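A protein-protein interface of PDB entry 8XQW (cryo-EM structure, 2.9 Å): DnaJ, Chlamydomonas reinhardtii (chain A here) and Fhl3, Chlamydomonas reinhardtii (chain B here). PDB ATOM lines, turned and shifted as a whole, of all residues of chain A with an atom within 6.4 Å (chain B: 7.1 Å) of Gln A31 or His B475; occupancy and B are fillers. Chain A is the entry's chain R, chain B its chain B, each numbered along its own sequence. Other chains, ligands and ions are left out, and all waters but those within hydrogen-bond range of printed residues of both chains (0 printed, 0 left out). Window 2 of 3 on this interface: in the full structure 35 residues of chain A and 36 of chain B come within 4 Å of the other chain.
Of the 12 printed residues of chain A, 5 touch a printed residue of chain B. Among the printed residues, 7 pairs touch across the chains. Among the printed residues, no Asp or Glu carboxylate lies within 4 Å of a Lys or Arg side-chain nitrogen of the other chain.
Ala A30 touches Leu B479. CB of His B475 touches CG2 of Ile A34 (3.6 Å). His B475 touches Trp A35. OE1 of Glu A38 touches CA of Ser B468, at 3.6 Å. Glu A38 touches Phe B471 (OE1 to CB, 3.3 Å). His B475 touches Glu A38 (NE2 to OE2, 3.9 Å).
The side-chain amide nitrogen (NE2) of Gln A31 lies within hydrogen-bond range of the backbone carbonyl oxygen (O) of His B475 (3.4 Å).
Of chain B, only His B475 comes within 4 Å of Gln A31. Printed residues of chain B within 4 Å of Ala A30: Leu B479 (3.9 Å). Of the printed residues of chain A, Leu B479 touches Ala A30. The nearest printed residue of chain A that does not touch His B475 is Ala A30 (6.4 Å).
A ring nitrogen (NE2) of His B475 sits close to the backbone carbonyl oxygen of Phe B471 (3.4 Å). The side-chain hydroxyl of Thr B476 is in hydrogen-bond range of a ring nitrogen (ND1) of His B475 (3.1 Å).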
ATOM      1  N   LEU A  26     -24.841   8.582 -30.748  1.00  0.00           N
ATOM      2  CA  LEU A  26     -23.531   8.876 -30.178  1.00  0.00           C
ATOM      3  C   LEU A  26     -23.645   9.230 -28.702  1.00  0.00           C
ATOM      4  O   LEU A  26     -22.874   8.732 -27.871  1.00  0.00           O
ATOM      5  CB  LEU A  26     -22.868  10.012 -30.950  1.00  0.00           C
ATOM      6  CG  LEU A  26     -22.416   9.694 -32.374  1.00  0.00           C
ATOM      7  CD1 LEU A  26     -21.738  10.904 -32.991  1.00  0.00           C
ATOM      8  CD2 LEU A  26     -21.496   8.492 -32.385  1.00  0.00           C
ATOM      9  N   VAL A  27     -24.600  10.097 -28.361  1.00  0.00           N
ATOM     10  CA  VAL A  27     -24.820  10.437 -26.959  1.00  0.00           C
ATOM     11  C   VAL A  27     -25.156   9.188 -26.159  1.00  0.00           C
ATOM     12  O   VAL A  27     -24.681   9.004 -25.031  1.00  0.00           O
ATOM     13  CB  VAL A  27     -25.924  11.501 -26.840  1.00  0.00           C
ATOM     14  CG1 VAL A  27     -26.354  11.660 -25.400  1.00  0.00           C
ATOM     15  CG2 VAL A  27     -25.441  12.821 -27.391  1.00  0.00           C
ATOM     16  N   TRP A  28     -25.964   8.303 -26.737  1.00  0.00           N
ATOM     17  CA  TRP A  28     -26.353   7.085 -26.042  1.00  0.00           C
ATOM     18  C   TRP A  28     -25.146   6.207 -25.747  1.00  0.00           C
ATOM     19  O   TRP A  28     -25.003   5.696 -24.632  1.00  0.00           O
ATOM     20  CB  TRP A  28     -27.381   6.330 -26.875  1.00  0.00           C
ATOM     21  CG  TRP A  28     -27.869   5.094 -26.240  1.00  0.00           C
ATOM     22  CD1 TRP A  28     -28.928   4.974 -25.400  1.00  0.00           C
ATOM     23  CD2 TRP A  28     -27.323   3.786 -26.390  1.00  0.00           C
ATOM     24  NE1 TRP A  28     -29.078   3.669 -25.014  1.00  0.00           N
ATOM     25  CE2 TRP A  28     -28.100   2.918 -25.610  1.00  0.00           C
ATOM     26  CE3 TRP A  28     -26.249   3.265 -27.106  1.00  0.00           C
ATOM     27  CZ2 TRP A  28     -27.841   1.560 -25.527  1.00  0.00           C
ATOM     28  CZ3 TRP A  28     -25.992   1.920 -27.023  1.00  0.00           C
ATOM     29  CH2 TRP A  28     -26.783   1.082 -26.240  1.00  0.00           C
ATOM     30  N   TRP A  29     -24.262   6.027 -26.726  1.00  0.00           N
ATOM     31  CA  TRP A  29     -23.084   5.190 -26.505  1.00  0.00           C
ATOM     32  C   TRP A  29     -22.155   5.797 -25.461  1.00  0.00           C
ATOM     33  O   TRP A  29     -21.647   5.088 -24.575  1.00  0.00           O
ATOM     34  CB  TRP A  29     -22.343   4.978 -27.820  1.00  0.00           C
ATOM     35  CG  TRP A  29     -22.947   3.924 -28.673  1.00  0.00           C
ATOM     36  CD1 TRP A  29     -23.897   4.090 -29.627  1.00  0.00           C
ATOM     37  CD2 TRP A  29     -22.638   2.530 -28.653  1.00  0.00           C
ATOM     38  NE1 TRP A  29     -24.202   2.887 -30.206  1.00  0.00           N
ATOM     39  CE2 TRP A  29     -23.439   1.912 -29.622  1.00  0.00           C
ATOM     40  CE3 TRP A  29     -21.756   1.743 -27.909  1.00  0.00           C
ATOM     41  CZ2 TRP A  29     -23.394   0.547 -29.866  1.00  0.00           C
ATOM     42  CZ3 TRP A  29     -21.712   0.391 -28.152  1.00  0.00           C
ATOM     43  CH2 TRP A  29     -22.523  -0.195 -29.121  1.00  0.00           C
ATOM     44  N   ALA A  30     -21.923   7.107 -25.541  1.00  0.00           N
ATOM     45  CA  ALA A  30     -21.085   7.763 -24.543  1.00  0.00           C
ATOM     46  C   ALA A  30     -21.638   7.552 -23.142  1.00  0.00           C
ATOM     47  O   ALA A  30     -20.909   7.151 -22.225  1.00  0.00           O
ATOM     48  CB  ALA A  30     -20.966   9.252 -24.850  1.00  0.00           C
ATOM     49  N   GLN A  31     -22.932   7.813 -22.957  1.00  0.00           N
ATOM     50  CA  GLN A  31     -23.517   7.662 -21.633  1.00  0.00           C
ATOM     51  C   GLN A  31     -23.476   6.214 -21.172  1.00  0.00           C
ATOM     52  O   GLN A  31     -23.237   5.938 -19.989  1.00  0.00           O
ATOM     53  CB  GLN A  31     -24.944   8.186 -21.635  1.00  0.00           C
ATOM     54  CG  GLN A  31     -25.012   9.678 -21.679  1.00  0.00           C
ATOM     55  CD  GLN A  31     -26.405  10.199 -21.469  1.00  0.00           C
ATOM     56  OE1 GLN A  31     -27.365   9.678 -22.030  1.00  0.00           O
ATOM     57  NE2 GLN A  31     -26.528  11.230 -20.653  1.00  0.00           N
ATOM     58  N   LYS A  32     -23.690   5.274 -22.089  1.00  0.00           N
ATOM     59  CA  LYS A  32     -23.715   3.873 -21.702  1.00  0.00           C
ATOM     60  C   LYS A  32     -22.332   3.379 -21.317  1.00  0.00           C
ATOM     61  O   LYS A  32     -22.199   2.322 -20.696  1.00  0.00           O
ATOM     62  CB  LYS A  32     -24.283   3.024 -22.831  1.00  0.00           C
ATOM     63  CG  LYS A  32     -24.933   1.749 -22.366  1.00  0.00           C
ATOM     64  CD  LYS A  32     -26.165   2.029 -21.550  1.00  0.00           C
ATOM     65  CE  LYS A  32     -27.039   0.796 -21.464  1.00  0.00           C
ATOM     66  NZ  LYS A  32     -26.263  -0.398 -21.049  1.00  0.00           N
ATOM     67  N   VAL A  33     -21.284   4.100 -21.702  1.00  0.00           N
ATOM     68  CA  VAL A  33     -19.970   3.705 -21.195  1.00  0.00           C
ATOM     69  C   VAL A  33     -19.658   4.427 -19.886  1.00  0.00           C
ATOM     70  O   VAL A  33     -19.051   3.853 -18.966  1.00  0.00           O
ATOM     71  CB  VAL A  33     -18.882   3.930 -22.264  1.00  0.00           C
ATOM     72  CG1 VAL A  33     -18.249   5.299 -22.145  1.00  0.00           C
ATOM     73  CG2 VAL A  33     -17.832   2.848 -22.173  1.00  0.00           C
ATOM     74  N   ILE A  34     -20.104   5.678 -19.759  1.00  0.00           N
ATOM     75  CA  ILE A  34     -19.753   6.452 -18.575  1.00  0.00           C
ATOM     76  C   ILE A  34     -20.451   5.893 -17.344  1.00  0.00           C
ATOM     77  O   ILE A  34     -19.865   5.830 -16.255  1.00  0.00           O
ATOM     78  CB  ILE A  34     -20.083   7.934 -18.793  1.00  0.00           C
ATOM     79  CG1 ILE A  34     -18.993   8.587 -19.635  1.00  0.00           C
ATOM     80  CG2 ILE A  34     -20.186   8.642 -17.475  1.00  0.00           C
ATOM     81  CD1 ILE A  34     -19.271  10.020 -19.988  1.00  0.00           C
ATOM     82  N   TRP A  35     -21.705   5.475 -17.491  1.00  0.00           N
ATOM     83  CA  TRP A  35     -22.423   4.908 -16.359  1.00  0.00           C
ATOM     84  C   TRP A  35     -21.736   3.661 -15.825  1.00  0.00           C
ATOM     85  O   TRP A  35     -21.665   3.461 -14.607  1.00  0.00           O
ATOM     86  CB  TRP A  35     -23.853   4.595 -16.766  1.00  0.00           C
ATOM     87  CG  TRP A  35     -24.677   5.812 -16.926  1.00  0.00           C
ATOM     88  CD1 TRP A  35     -24.536   6.981 -16.253  1.00  0.00           C
ATOM     89  CD2 TRP A  35     -25.771   5.990 -17.817  1.00  0.00           C
ATOM     90  NE1 TRP A  35     -25.480   7.880 -16.667  1.00  0.00           N
ATOM     91  CE2 TRP A  35     -26.253   7.292 -17.629  1.00  0.00           C
ATOM     92  CE3 TRP A  35     -26.397   5.172 -18.757  1.00  0.00           C
ATOM     93  CZ2 TRP A  35     -27.326   7.797 -18.344  1.00  0.00           C
ATOM     94  CZ3 TRP A  35     -27.461   5.676 -19.468  1.00  0.00           C
ATOM     95  CH2 TRP A  35     -27.917   6.973 -19.257  1.00  0.00           C
ATOM     96  N   LEU A  36     -21.206   2.827 -16.711  1.00  0.00           N
ATOM     97  CA  LEU A  36     -20.506   1.632 -16.265  1.00  0.00           C
ATOM     98  C   LEU A  36     -19.201   1.986 -15.565  1.00  0.00           C
ATOM     99  O   LEU A  36     -18.832   1.346 -14.572  1.00  0.00           O
ATOM    100  CB  LEU A  36     -20.256   0.718 -17.455  1.00  0.00           C
ATOM    101  CG  LEU A  36     -19.737  -0.672 -17.135  1.00  0.00           C
ATOM    102  CD1 LEU A  36     -20.601  -1.298 -16.085  1.00  0.00           C
ATOM    103  CD2 LEU A  36     -19.748  -1.502 -18.388  1.00  0.00           C
ATOM    104  N   GLU A  38     -18.769   4.608 -13.774  1.00  0.00           N
ATOM    105  CA  GLU A  38     -19.178   5.083 -12.457  1.00  0.00           C
ATOM    106  C   GLU A  38     -19.548   3.929 -11.537  1.00  0.00           C
ATOM    107  O   GLU A  38     -19.249   3.960 -10.340  1.00  0.00           O
ATOM    108  CB  GLU A  38     -20.350   6.040 -12.604  1.00  0.00           C
ATOM    109  CG  GLU A  38     -20.714   6.769 -11.351  1.00  0.00           C
ATOM    110  CD  GLU A  38     -21.915   7.662 -11.550  1.00  0.00           C
ATOM    111  OE1 GLU A  38     -22.134   8.566 -10.725  1.00  0.00           O
ATOM    112  OE2 GLU A  38     -22.644   7.460 -12.540  1.00  0.00           O
ATOM    113  N   SER B 468     -20.906  10.550  -6.989  1.00  0.00           N
ATOM    114  CA  SER B 468     -22.057  10.749  -7.855  1.00  0.00           C
ATOM    115  C   SER B 468     -22.093  12.156  -8.419  1.00  0.00           C
ATOM    116  O   SER B 468     -22.414  12.333  -9.591  1.00  0.00           O
ATOM    117  CB  SER B 468     -23.343  10.452  -7.098  1.00  0.00           C
ATOM    118  OG  SER B 468     -23.942  11.652  -6.656  1.00  0.00           O
ATOM    119  N   LEU B 470     -19.520  14.159  -9.035  1.00  0.00           N
ATOM    120  CA  LEU B 470     -18.473  14.305 -10.041  1.00  0.00           C
ATOM    121  C   LEU B 470     -18.885  13.671 -11.368  1.00  0.00           C
ATOM    122  O   LEU B 470     -18.824  14.310 -12.435  1.00  0.00           O
ATOM    123  CB  LEU B 470     -17.182  13.692  -9.509  1.00  0.00           C
ATOM    124  CG  LEU B 470     -15.977  13.557 -10.420  1.00  0.00           C
ATOM    125  CD1 LEU B 470     -14.802  14.248  -9.791  1.00  0.00           C
ATOM    126  CD2 LEU B 470     -15.662  12.101 -10.601  1.00  0.00           C
ATOM    127  N   PHE B 471     -19.329  12.418 -11.325  1.00  0.00           N
ATOM    128  CA  PHE B 471     -19.723  11.787 -12.577  1.00  0.00           C
ATOM    129  C   PHE B 471     -20.969  12.432 -13.165  1.00  0.00           C
ATOM    130  O   PHE B 471     -21.136  12.437 -14.389  1.00  0.00           O
ATOM    131  CB  PHE B 471     -19.934  10.298 -12.380  1.00  0.00           C
ATOM    132  CG  PHE B 471     -18.676   9.510 -12.466  1.00  0.00           C
ATOM    133  CD1 PHE B 471     -17.893   9.320 -11.352  1.00  0.00           C
ATOM    134  CD2 PHE B 471     -18.264   8.977 -13.663  1.00  0.00           C
ATOM    135  CE1 PHE B 471     -16.738   8.604 -11.426  1.00  0.00           C
ATOM    136  CE2 PHE B 471     -17.104   8.262 -13.741  1.00  0.00           C
ATOM    137  CZ  PHE B 471     -16.342   8.075 -12.621  1.00  0.00           C
ATOM    138  N   TRP B 472     -21.845  12.988 -12.331  1.00  0.00           N
ATOM    139  CA  TRP B 472     -22.994  13.707 -12.859  1.00  0.00           C
ATOM    140  C   TRP B 472     -22.546  14.928 -13.626  1.00  0.00           C
ATOM    141  O   TRP B 472     -23.020  15.183 -14.734  1.00  0.00           O
ATOM    142  CB  TRP B 472     -23.937  14.123 -11.738  1.00  0.00           C
ATOM    143  CG  TRP B 472     -24.980  15.072 -12.206  1.00  0.00           C
ATOM    144  CD1 TRP B 472     -26.192  14.753 -12.723  1.00  0.00           C
ATOM    145  CD2 TRP B 472     -24.904  16.499 -12.215  1.00  0.00           C
ATOM    146  NE1 TRP B 472     -26.880  15.888 -13.050  1.00  0.00           N
ATOM    147  CE2 TRP B 472     -26.107  16.976 -12.747  1.00  0.00           C
ATOM    148  CE3 TRP B 472     -23.934  17.420 -11.822  1.00  0.00           C
ATOM    149  CZ2 TRP B 472     -26.369  18.326 -12.896  1.00  0.00           C
ATOM    150  CZ3 TRP B 472     -24.194  18.758 -11.978  1.00  0.00           C
ATOM    151  CH2 TRP B 472     -25.401  19.200 -12.507  1.00  0.00           C
ATOM    152  N   MET B 473     -21.658  15.723 -13.031  1.00  0.00           N
ATOM    153  CA  MET B 473     -21.086  16.851 -13.746  1.00  0.00           C
ATOM    154  C   MET B 473     -20.677  16.421 -15.137  1.00  0.00           C
ATOM    155  O   MET B 473     -21.214  16.914 -16.135  1.00  0.00           O
ATOM    156  CB  MET B 473     -19.892  17.412 -12.985  1.00  0.00           C
ATOM    157  CG  MET B 473     -19.832  18.911 -12.973  1.00  0.00           C
ATOM    158  SD  MET B 473     -19.086  19.534 -11.462  1.00  0.00           S
ATOM    159  CE  MET B 473     -17.475  18.759 -11.547  1.00  0.00           C
ATOM    160  N   ILE B 474     -19.803  15.416 -15.213  1.00  0.00           N
ATOM    161  CA  ILE B 474     -19.284  14.988 -16.516  1.00  0.00           C
ATOM    162  C   ILE B 474     -20.422  14.607 -17.462  1.00  0.00           C
ATOM    163  O   ILE B 474     -20.590  15.210 -18.525  1.00  0.00           O
ATOM    164  CB  ILE B 474     -18.287  13.832 -16.360  1.00  0.00           C
ATOM    165  CG1 ILE B 474     -16.930  14.353 -15.911  1.00  0.00           C
ATOM    166  CG2 ILE B 474     -18.119  13.114 -17.673  1.00  0.00           C
ATOM    167  CD1 ILE B 474     -15.864  13.297 -15.915  1.00  0.00           C
ATOM    168  N   HIS B 475     -21.225  13.607 -17.093  1.00  0.00           N
ATOM    169  CA  HIS B 475     -22.105  13.000 -18.088  1.00  0.00           C
ATOM    170  C   HIS B 475     -23.457  13.679 -18.231  1.00  0.00           C
ATOM    171  O   HIS B 475     -24.272  13.208 -19.027  1.00  0.00           O
ATOM    172  CB  HIS B 475     -22.327  11.507 -17.798  1.00  0.00           C
ATOM    173  CG  HIS B 475     -23.107  11.217 -16.550  1.00  0.00           C
ATOM    174  ND1 HIS B 475     -24.306  11.824 -16.249  1.00  0.00           N
ATOM    175  CD2 HIS B 475     -22.866  10.350 -15.539  1.00  0.00           C
ATOM    176  CE1 HIS B 475     -24.757  11.362 -15.098  1.00  0.00           C
ATOM    177  NE2 HIS B 475     -23.902  10.466 -14.646  1.00  0.00           N
ATOM    178  N   THR B 476     -23.755  14.717 -17.472  1.00  0.00           N
ATOM    179  CA  THR B 476     -25.017  15.406 -17.686  1.00  0.00           C
ATOM    180  C   THR B 476     -24.882  16.916 -17.754  1.00  0.00           C
ATOM    181  O   THR B 476     -25.538  17.545 -18.585  1.00  0.00           O
ATOM    182  CB  THR B 476     -26.013  15.017 -16.592  1.00  0.00           C
ATOM    183  OG1 THR B 476     -26.598  13.755 -16.923  1.00  0.00           O
ATOM    184  CG2 THR B 476     -27.111  16.048 -16.459  1.00  0.00           C
ATOM    185  N   TRP B 477     -24.029  17.527 -16.934  1.00  0.00           N
ATOM    186  CA  TRP B 477     -23.933  18.975 -17.013  1.00  0.00           C
ATOM    187  C   TRP B 477     -23.206  19.416 -18.267  1.00  0.00           C
ATOM    188  O   TRP B 477     -23.271  20.593 -18.630  1.00  0.00           O
ATOM    189  CB  TRP B 477     -23.236  19.530 -15.780  1.00  0.00           C
ATOM    190  CG  TRP B 477     -23.236  21.006 -15.739  1.00  0.00           C
ATOM    191  CD1 TRP B 477     -24.273  21.815 -15.405  1.00  0.00           C
ATOM    192  CD2 TRP B 477     -22.143  21.864 -16.066  1.00  0.00           C
ATOM    193  NE1 TRP B 477     -23.896  23.130 -15.490  1.00  0.00           N
ATOM    194  CE2 TRP B 477     -22.589  23.186 -15.898  1.00  0.00           C
ATOM    195  CE3 TRP B 477     -20.830  21.643 -16.482  1.00  0.00           C
ATOM    196  CZ2 TRP B 477     -21.769  24.283 -16.131  1.00  0.00           C
ATOM    197  CZ3 TRP B 477     -20.017  22.732 -16.713  1.00  0.00           C
ATOM    198  CH2 TRP B 477     -20.490  24.037 -16.537  1.00  0.00           C
ATOM    199  N   ILE B 478     -22.519  18.498 -18.937  1.00  0.00           N
ATOM    200  CA  ILE B 478     -21.888  18.774 -20.218  1.00  0.00           C
ATOM    201  C   ILE B 478     -22.719  18.111 -21.305  1.00  0.00           C
ATOM    202  O   ILE B 478     -23.258  18.785 -22.190  1.00  0.00           O
ATOM    203  CB  ILE B 478     -20.438  18.269 -20.243  1.00  0.00           C
ATOM    204  CG1 ILE B 478     -19.572  19.105 -19.310  1.00  0.00           C
ATOM    205  CG2 ILE B 478     -19.893  18.337 -21.636  1.00  0.00           C
ATOM    206  CD1 ILE B 478     -18.105  18.835 -19.465  1.00  0.00           C
ATOM    207  N   LEU B 479     -22.851  16.790 -21.228  1.00  0.00           N
ATOM    208  CA  LEU B 479     -23.610  16.012 -22.205  1.00  0.00           C
ATOM    209  C   LEU B 479     -25.112  16.121 -21.940  1.00  0.00           C
ATOM    210  O   LEU B 479     -25.818  15.128 -21.775  1.00  0.00           O
ATOM    211  CB  LEU B 479     -23.164  14.559 -22.168  1.00  0.00           C
ATOM    212  CG  LEU B 479     -22.372  14.045 -23.352  1.00  0.00           C
ATOM    213  CD1 LEU B 479     -22.535  12.546 -23.442  1.00  0.00           C
ATOM    214  CD2 LEU B 479     -22.863  14.712 -24.604  1.00  0.00           C
ATOM    215  N   ASP B 480     -25.592  17.360 -21.910  1.00  0.00           N
ATOM    216  CA  ASP B 480     -26.973  17.652 -21.545  1.00  0.00           C
ATOM    217  C   ASP B 480     -27.980  16.861 -22.374  1.00  0.00           C
ATOM    218  O   ASP B 480     -28.467  15.819 -21.938  1.00  0.00           O
ATOM    219  CB  ASP B 480     -27.251  19.146 -21.688  1.00  0.00           C
ATOM    220  CG  ASP B 480     -28.562  19.554 -21.061  1.00  0.00           C
ATOM    221  OD1 ASP B 480     -29.084  18.787 -20.221  1.00  0.00           O
ATOM    222  OD2 ASP B 480     -29.073  20.636 -21.412  1.00  0.00           O
